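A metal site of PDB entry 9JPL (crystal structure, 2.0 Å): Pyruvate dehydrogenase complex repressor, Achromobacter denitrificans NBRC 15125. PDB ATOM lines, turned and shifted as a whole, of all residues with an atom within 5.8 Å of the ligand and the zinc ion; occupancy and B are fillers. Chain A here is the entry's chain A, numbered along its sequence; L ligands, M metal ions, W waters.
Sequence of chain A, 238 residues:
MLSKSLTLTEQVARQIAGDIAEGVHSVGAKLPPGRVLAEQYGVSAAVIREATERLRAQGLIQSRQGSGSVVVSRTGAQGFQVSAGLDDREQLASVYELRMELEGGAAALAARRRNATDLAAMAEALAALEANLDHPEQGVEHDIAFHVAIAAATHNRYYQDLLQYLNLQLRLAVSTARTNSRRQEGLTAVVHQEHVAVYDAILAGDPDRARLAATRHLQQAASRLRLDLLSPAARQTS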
ATOM      1  N   TYR A  96      -0.275   2.934  27.722  1.00  0.00           N
ATOM      2  CA  TYR A  96       0.517   3.469  28.819  1.00  0.00           C
ATOM      3  C   TYR A  96       0.736   2.426  29.919  1.00  0.00           C
ATOM      4  O   TYR A  96       1.834   2.362  30.488  1.00  0.00           O
ATOM      5  CB  TYR A  96      -0.133   4.753  29.363  1.00  0.00           C
ATOM      6  CG  TYR A  96       0.353   5.958  28.560  1.00  0.00           C
ATOM      7  CD1 TYR A  96       1.671   6.413  28.676  1.00  0.00           C
ATOM      8  CD2 TYR A  96      -0.488   6.617  27.667  1.00  0.00           C
ATOM      9  CE1 TYR A  96       2.123   7.489  27.924  1.00  0.00           C
ATOM     10  CE2 TYR A  96      -0.042   7.701  26.905  1.00  0.00           C
ATOM     11  CZ  TYR A  96       1.267   8.130  27.036  1.00  0.00           C
ATOM     12  OH  TYR A  96       1.717   9.199  26.291  1.00  0.00           O
ATOM     13  N   ARG A  99       3.555   0.236  28.545  1.00  0.00           N
ATOM     14  CA  ARG A  99       4.806   0.992  28.540  1.00  0.00           C
ATOM     15  C   ARG A  99       5.391   1.088  29.941  1.00  0.00           C
ATOM     16  O   ARG A  99       6.606   1.039  30.115  1.00  0.00           O
ATOM     17  CB  ARG A  99       4.562   2.390  27.960  1.00  0.00           C
ATOM     18  CG  ARG A  99       4.411   2.415  26.429  1.00  0.00           C
ATOM     19  CD  ARG A  99       4.207   3.836  25.904  1.00  0.00           C
ATOM     20  NE  ARG A  99       5.464   4.586  25.982  1.00  0.00           N
ATOM     21  CZ  ARG A  99       5.558   5.907  25.863  1.00  0.00           C
ATOM     22  NH1 ARG A  99       4.459   6.639  25.643  1.00  0.00           N
ATOM     23  NH2 ARG A  99       6.754   6.488  25.958  1.00  0.00           N
ATOM     24  N   GLU A 103       8.936  -0.159  29.771  1.00  0.00           N
ATOM     25  CA  GLU A 103       9.932   0.902  29.784  1.00  0.00           C
ATOM     26  C   GLU A 103      10.518   1.127  31.176  1.00  0.00           C
ATOM     27  O   GLU A 103      11.675   1.535  31.280  1.00  0.00           O
ATOM     28  CB  GLU A 103       9.341   2.219  29.238  1.00  0.00           C
ATOM     29  CG  GLU A 103       9.082   2.140  27.736  1.00  0.00           C
ATOM     30  CD  GLU A 103       8.489   3.426  27.103  1.00  0.00           C
ATOM     31  OE1 GLU A 103       8.770   4.548  27.581  1.00  0.00           O
ATOM     32  OE2 GLU A 103       7.731   3.282  26.128  1.00  0.00           O
ATOM     33  N   ASP A 143      10.862  12.130  20.615  1.00  0.00           N
ATOM     34  CA  ASP A 143      10.362  11.533  21.850  1.00  0.00           C
ATOM     35  C   ASP A 143      10.410  10.013  21.772  1.00  0.00           C
ATOM     36  O   ASP A 143      10.983   9.352  22.649  1.00  0.00           O
ATOM     37  CB  ASP A 143       8.919  12.045  22.079  1.00  0.00           C
ATOM     38  CG  ASP A 143       8.408  11.870  23.531  1.00  0.00           C
ATOM     39  OD1 ASP A 143       8.711  10.852  24.174  1.00  0.00           O
ATOM     40  OD2 ASP A 143       7.633  12.756  24.009  1.00  0.00           O
ATOM     41  N   PHE A 146      14.019   8.723  21.763  1.00  0.00           N
ATOM     42  CA  PHE A 146      14.605   8.703  23.099  1.00  0.00           C
ATOM     43  C   PHE A 146      14.219   7.424  23.847  1.00  0.00           C
ATOM     44  O   PHE A 146      15.079   6.731  24.402  1.00  0.00           O
ATOM     45  CB  PHE A 146      14.167   9.953  23.874  1.00  0.00           C
ATOM     46  CG  PHE A 146      14.610   9.965  25.322  1.00  0.00           C
ATOM     47  CD1 PHE A 146      15.935  10.275  25.664  1.00  0.00           C
ATOM     48  CD2 PHE A 146      13.707   9.662  26.357  1.00  0.00           C
ATOM     49  CE1 PHE A 146      16.344  10.290  27.014  1.00  0.00           C
ATOM     50  CE2 PHE A 146      14.119   9.684  27.700  1.00  0.00           C
ATOM     51  CZ  PHE A 146      15.439   9.986  28.019  1.00  0.00           C
ATOM     52  N   HIS A 147      12.933   7.067  23.851  1.00  0.00           N
ATOM     53  CA  HIS A 147      12.505   5.857  24.560  1.00  0.00           C
ATOM     54  C   HIS A 147      13.060   4.606  23.891  1.00  0.00           C
ATOM     55  O   HIS A 147      13.467   3.666  24.580  1.00  0.00           O
ATOM     56  CB  HIS A 147      10.981   5.819  24.643  1.00  0.00           C
ATOM     57  CG  HIS A 147      10.407   6.940  25.456  1.00  0.00           C
ATOM     58  ND1 HIS A 147      10.641   7.055  26.809  1.00  0.00           N
ATOM     59  CD2 HIS A 147       9.694   8.023  25.098  1.00  0.00           C
ATOM     60  CE1 HIS A 147      10.067   8.166  27.254  1.00  0.00           C
ATOM     61  NE2 HIS A 147       9.483   8.760  26.238  1.00  0.00           N
ATOM     62  N   ALA A 173       0.207   7.137  21.200  1.00  0.00           N
ATOM     63  CA  ALA A 173       0.249   7.660  22.552  1.00  0.00           C
ATOM     64  C   ALA A 173       1.039   8.970  22.606  1.00  0.00           C
ATOM     65  O   ALA A 173       0.566   9.962  23.184  1.00  0.00           O
ATOM     66  CB  ALA A 173       0.874   6.635  23.498  1.00  0.00           C
ATOM     67  N   VAL A 174       2.240   8.973  22.023  1.00  0.00           N
ATOM     68  CA  VAL A 174       3.120  10.141  22.127  1.00  0.00           C
ATOM     69  C   VAL A 174       2.539  11.336  21.372  1.00  0.00           C
ATOM     70  O   VAL A 174       2.590  12.480  21.857  1.00  0.00           O
ATOM     71  CB  VAL A 174       4.533   9.785  21.643  1.00  0.00           C
ATOM     72  CG1 VAL A 174       5.398  11.049  21.487  1.00  0.00           C
ATOM     73  CG2 VAL A 174       5.236   8.756  22.605  1.00  0.00           C
ATOM     74  N   ALA A 177      -0.349  12.705  23.469  1.00  0.00           N
ATOM     75  CA  ALA A 177       0.154  13.353  24.676  1.00  0.00           C
ATOM     76  C   ALA A 177       0.777  14.708  24.386  1.00  0.00           C
ATOM     77  O   ALA A 177       0.478  15.696  25.050  1.00  0.00           O
ATOM     78  CB  ALA A 177       1.171  12.439  25.379  1.00  0.00           C
ATOM     79  N   ARG A 178       1.668  14.770  23.380  1.00  0.00           N
ATOM     80  CA  ARG A 178       2.384  16.019  23.147  1.00  0.00           C
ATOM     81  C   ARG A 178       1.442  17.113  22.643  1.00  0.00           C
ATOM     82  O   ARG A 178       1.549  18.267  23.048  1.00  0.00           O
ATOM     83  CB  ARG A 178       3.546  15.783  22.179  1.00  0.00           C
ATOM     84  CG  ARG A 178       4.633  14.833  22.764  1.00  0.00           C
ATOM     85  CD  ARG A 178       5.784  14.626  21.776  1.00  0.00           C
ATOM     86  NE  ARG A 178       6.535  15.872  21.641  1.00  0.00           N
ATOM     87  CZ  ARG A 178       7.488  16.261  22.469  1.00  0.00           C
ATOM     88  NH1 ARG A 178       7.844  15.480  23.485  1.00  0.00           N
ATOM     89  NH2 ARG A 178       8.086  17.422  22.274  1.00  0.00           N
ATOM     90  N   SER A 181      -0.296  18.391  25.694  1.00  0.00           N
ATOM     91  CA  SER A 181       0.526  19.189  26.604  1.00  0.00           C
ATOM     92  C   SER A 181       0.816  20.590  26.071  1.00  0.00           C
ATOM     93  O   SER A 181       1.031  21.522  26.860  1.00  0.00           O
ATOM     94  CB  SER A 181       1.843  18.468  26.914  1.00  0.00           C
ATOM     95  OG  SER A 181       1.605  17.332  27.730  1.00  0.00           O
ATOM     96  N   VAL A 191       7.462  18.461  30.925  1.00  0.00           N
ATOM     97  CA  VAL A 191       7.590  17.116  30.372  1.00  0.00           C
ATOM     98  C   VAL A 191       9.035  16.850  29.971  1.00  0.00           C
ATOM     99  O   VAL A 191       9.550  15.743  30.164  1.00  0.00           O
ATOM    100  CB  VAL A 191       6.619  16.922  29.200  1.00  0.00           C
ATOM    101  CG1 VAL A 191       6.913  15.595  28.449  1.00  0.00           C
ATOM    102  CG2 VAL A 191       5.209  16.928  29.747  1.00  0.00           C
ATOM    103  N   GLU A 194      10.984  15.479  32.697  1.00  0.00           N
ATOM    104  CA  GLU A 194      10.711  14.067  32.912  1.00  0.00           C
ATOM    105  C   GLU A 194      11.640  13.183  32.086  1.00  0.00           C
ATOM    106  O   GLU A 194      12.104  12.142  32.562  1.00  0.00           O
ATOM    107  CB  GLU A 194       9.238  13.731  32.596  1.00  0.00           C
ATOM    108  CG  GLU A 194       8.228  14.451  33.506  1.00  0.00           C
ATOM    109  CD  GLU A 194       6.777  14.279  33.053  1.00  0.00           C
ATOM    110  OE1 GLU A 194       6.474  13.451  32.151  1.00  0.00           O
ATOM    111  OE2 GLU A 194       5.919  14.995  33.623  1.00  0.00           O
ATOM    112  N   HIS A 195      11.905  13.573  30.830  1.00  0.00           N
ATOM    113  CA  HIS A 195      12.865  12.828  30.004  1.00  0.00           C
ATOM    114  C   HIS A 195      14.283  12.964  30.553  1.00  0.00           C
ATOM    115  O   HIS A 195      15.038  11.987  30.569  1.00  0.00           O
ATOM    116  CB  HIS A 195      12.834  13.309  28.548  1.00  0.00           C
ATOM    117  CG  HIS A 195      11.605  12.916  27.797  1.00  0.00           C
ATOM    118  ND1 HIS A 195      10.988  13.747  26.873  1.00  0.00           N
ATOM    119  CD2 HIS A 195      10.856  11.789  27.844  1.00  0.00           C
ATOM    120  CE1 HIS A 195       9.922  13.135  26.390  1.00  0.00           C
ATOM    121  NE2 HIS A 195       9.822  11.941  26.954  1.00  0.00           N
ATOM    122  N   HIS A 217       7.315   9.221  34.475  1.00  0.00           N
ATOM    123  CA  HIS A 217       7.037   9.933  33.228  1.00  0.00           C
ATOM    124  C   HIS A 217       5.747   9.431  32.593  1.00  0.00           C
ATOM    125  O   HIS A 217       4.900  10.225  32.152  1.00  0.00           O
ATOM    126  CB  HIS A 217       8.243   9.762  32.282  1.00  0.00           C
ATOM    127  CG  HIS A 217       7.995  10.199  30.864  1.00  0.00           C
ATOM    128  ND1 HIS A 217       7.514  11.447  30.516  1.00  0.00           N
ATOM    129  CD2 HIS A 217       8.254   9.568  29.686  1.00  0.00           C
ATOM    130  CE1 HIS A 217       7.449  11.557  29.202  1.00  0.00           C
ATOM    131  NE2 HIS A 217       7.898  10.427  28.672  1.00  0.00           N
ATOM    132  N   LEU A 218       5.561   8.106  32.554  1.00  0.00           N
ATOM    133  CA  LEU A 218       4.392   7.527  31.899  1.00  0.00           C
ATOM    134  C   LEU A 218       3.132   7.712  32.747  1.00  0.00           C
ATOM    135  O   LEU A 218       2.036   7.912  32.205  1.00  0.00           O
ATOM    136  CB  LEU A 218       4.662   6.059  31.593  1.00  0.00           C
ATOM    137  CG  LEU A 218       5.888   5.871  30.683  1.00  0.00           C
ATOM    138  CD1 LEU A 218       6.322   4.427  30.657  1.00  0.00           C
ATOM    139  CD2 LEU A 218       5.605   6.392  29.243  1.00  0.00           C
ATOM    140  N   GLN A 220       2.582  10.342  34.718  1.00  0.00           N
ATOM    141  CA  GLN A 220       2.186  11.740  34.589  1.00  0.00           C
ATOM    142  C   GLN A 220       1.561  12.009  33.225  1.00  0.00           C
ATOM    143  O   GLN A 220       0.614  12.799  33.124  1.00  0.00           O
ATOM    144  CB  GLN A 220       3.397  12.638  34.828  1.00  0.00           C
ATOM    145  CG  GLN A 220       3.914  12.559  36.267  1.00  0.00           C
ATOM    146  CD  GLN A 220       2.839  12.948  37.270  1.00  0.00           C
ATOM    147  OE1 GLN A 220       2.433  12.147  38.111  1.00  0.00           O
ATOM    148  NE2 GLN A 220       2.364  14.180  37.182  1.00  0.00           N
ATOM    149  N   ALA A 221       2.091  11.382  32.166  1.00  0.00           N
ATOM    150  CA  ALA A 221       1.488  11.527  30.839  1.00  0.00           C
ATOM    151  C   ALA A 221       0.064  10.991  30.831  1.00  0.00           C
ATOM    152  O   ALA A 221      -0.850  11.620  30.280  1.00  0.00           O
ATOM    153  CB  ALA A 221       2.347  10.813  29.798  1.00  0.00           C
ATOM    154  N   ARG A 224      -2.018  13.495  32.728  1.00  0.00           N
ATOM    155  CA  ARG A 224      -2.305  14.678  31.931  1.00  0.00           C
ATOM    156  C   ARG A 224      -3.443  14.436  30.944  1.00  0.00           C
ATOM    157  O   ARG A 224      -4.222  15.345  30.654  1.00  0.00           O
ATOM    158  CB  ARG A 224      -1.058  15.128  31.166  1.00  0.00           C
ATOM    159  CG  ARG A 224      -0.029  15.863  32.020  1.00  0.00           C
ATOM    160  CD  ARG A 224       1.119  16.368  31.151  1.00  0.00           C
ATOM    161  NE  ARG A 224       2.053  15.316  30.729  1.00  0.00           N
ATOM    162  CZ  ARG A 224       3.082  14.880  31.453  1.00  0.00           C
ATOM    163  NH1 ARG A 224       3.311  15.378  32.659  1.00  0.00           N
ATOM    164  NH2 ARG A 224       3.880  13.940  30.977  1.00  0.00           N
HETATM  165  C1  LIG L   1       5.537  10.004  26.046  1.00  0.00           C
HETATM  166  O1  LIG L   1       4.476   9.347  26.067  1.00  0.00           O
HETATM  167  C2  LIG L   1       5.516  11.529  25.924  1.00  0.00           C
HETATM  168  O2  LIG L   1       6.649   9.393  26.069  1.00  0.00           O
HETATM  169  C3  LIG L   1       4.495  12.229  26.825  1.00  0.00           C
HETATM  170  O3  LIG L   1       6.807  12.022  26.222  1.00  0.00           O
HETATM  171  C4  LIG L   1       4.464  13.696  26.345  1.00  0.00           C
HETATM  172  O4  LIG L   1       2.934  14.014  28.190  1.00  0.00           O
HETATM  173  C5  LIG L   1       3.515  14.526  27.212  1.00  0.00           C
HETATM  174  O5  LIG L   1       3.303  15.748  26.941  1.00  0.00           O
HETATM  175 ZN    ZN M   1       8.323  10.503  26.489  1.00  0.00          ZN
HETATM  176  O   HOH W   1       5.122  17.174  25.613  1.00  0.00           O
HETATM  177  O   HOH W   2       0.135  13.599  28.377  1.00  0.00           O
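The backbone carbonyl oxygen (O) of Ala 177 sits close to an oxygen (O5) of the ligand (3.4 Å). Merely in contact with the ligand: Val 191 (3.6 Å), Val 174 (3.6 Å), Ala 221 (3.6 Å) and Arg 178 (3.8 Å). Of the 19 residues printed, 13 come within 4 Å of the ligand. The nearest printed residue that does not touch the ligand is Leu 218 (4.5 Å).
The zinc ion is bound by O2 of the ligand, NE2 of His 147, NE2 of His 195, O3 of the ligand, NE2 of His 217 and OD1 of Asp 143.
The nearest printed residue that does not touch the zinc ion is Arg 99 (4.3 Å).
The guanidinium group of Arg 224 lies within salt-bridge range of an oxygen (O4) of the ligand (2.9 Å). The side-chain hydroxyl of Tyr 96 is in hydrogen-bond range of an oxygen (O1) of the ligand (2.8 Å). An oxygen (O5) of the ligand sits at hydrogen-bond distance from the side-chain hydroxyl of Ser 181. The guanidinium group of Arg 99 is in salt-bridge range of an oxygen (O1) of the ligand (2.7 Å).
OH of Tyr 96 is in hydrogen-bond range of O of Ala 173 (3.4 Å). ND1 of His 217 sits at hydrogen-bond distance from OE1 of Glu 194, at 2.8 Å. The guanidinium group of Arg 178 lies within salt-bridge range of the side-chain carboxylate of Asp 143 (2.8 Å). ND1 of His 147 lies within hydrogen-bond range of OE1 of Glu 103 (3.2 Å). The guanidinium group (NH1) of Arg 224 lies within salt-bridge range of the side-chain carboxylate (OE2) of Glu 194 (2.8 Å). OG of Ser 181 lies within hydrogen-bond range of O of Ala 177 (3.3 Å). The guanidinium group of Arg 99 lies within salt-bridge range of the side-chain carboxylate of Glu 103 (2.6 Å).
Water W2 lies within hydrogen-bond range of an oxygen (O4) of the ligand (2.8 Å), the backbone carbonyl oxygen of Ala 221 (2.9 Å) and the guanidinium group of Arg 224 (3.5 Å).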
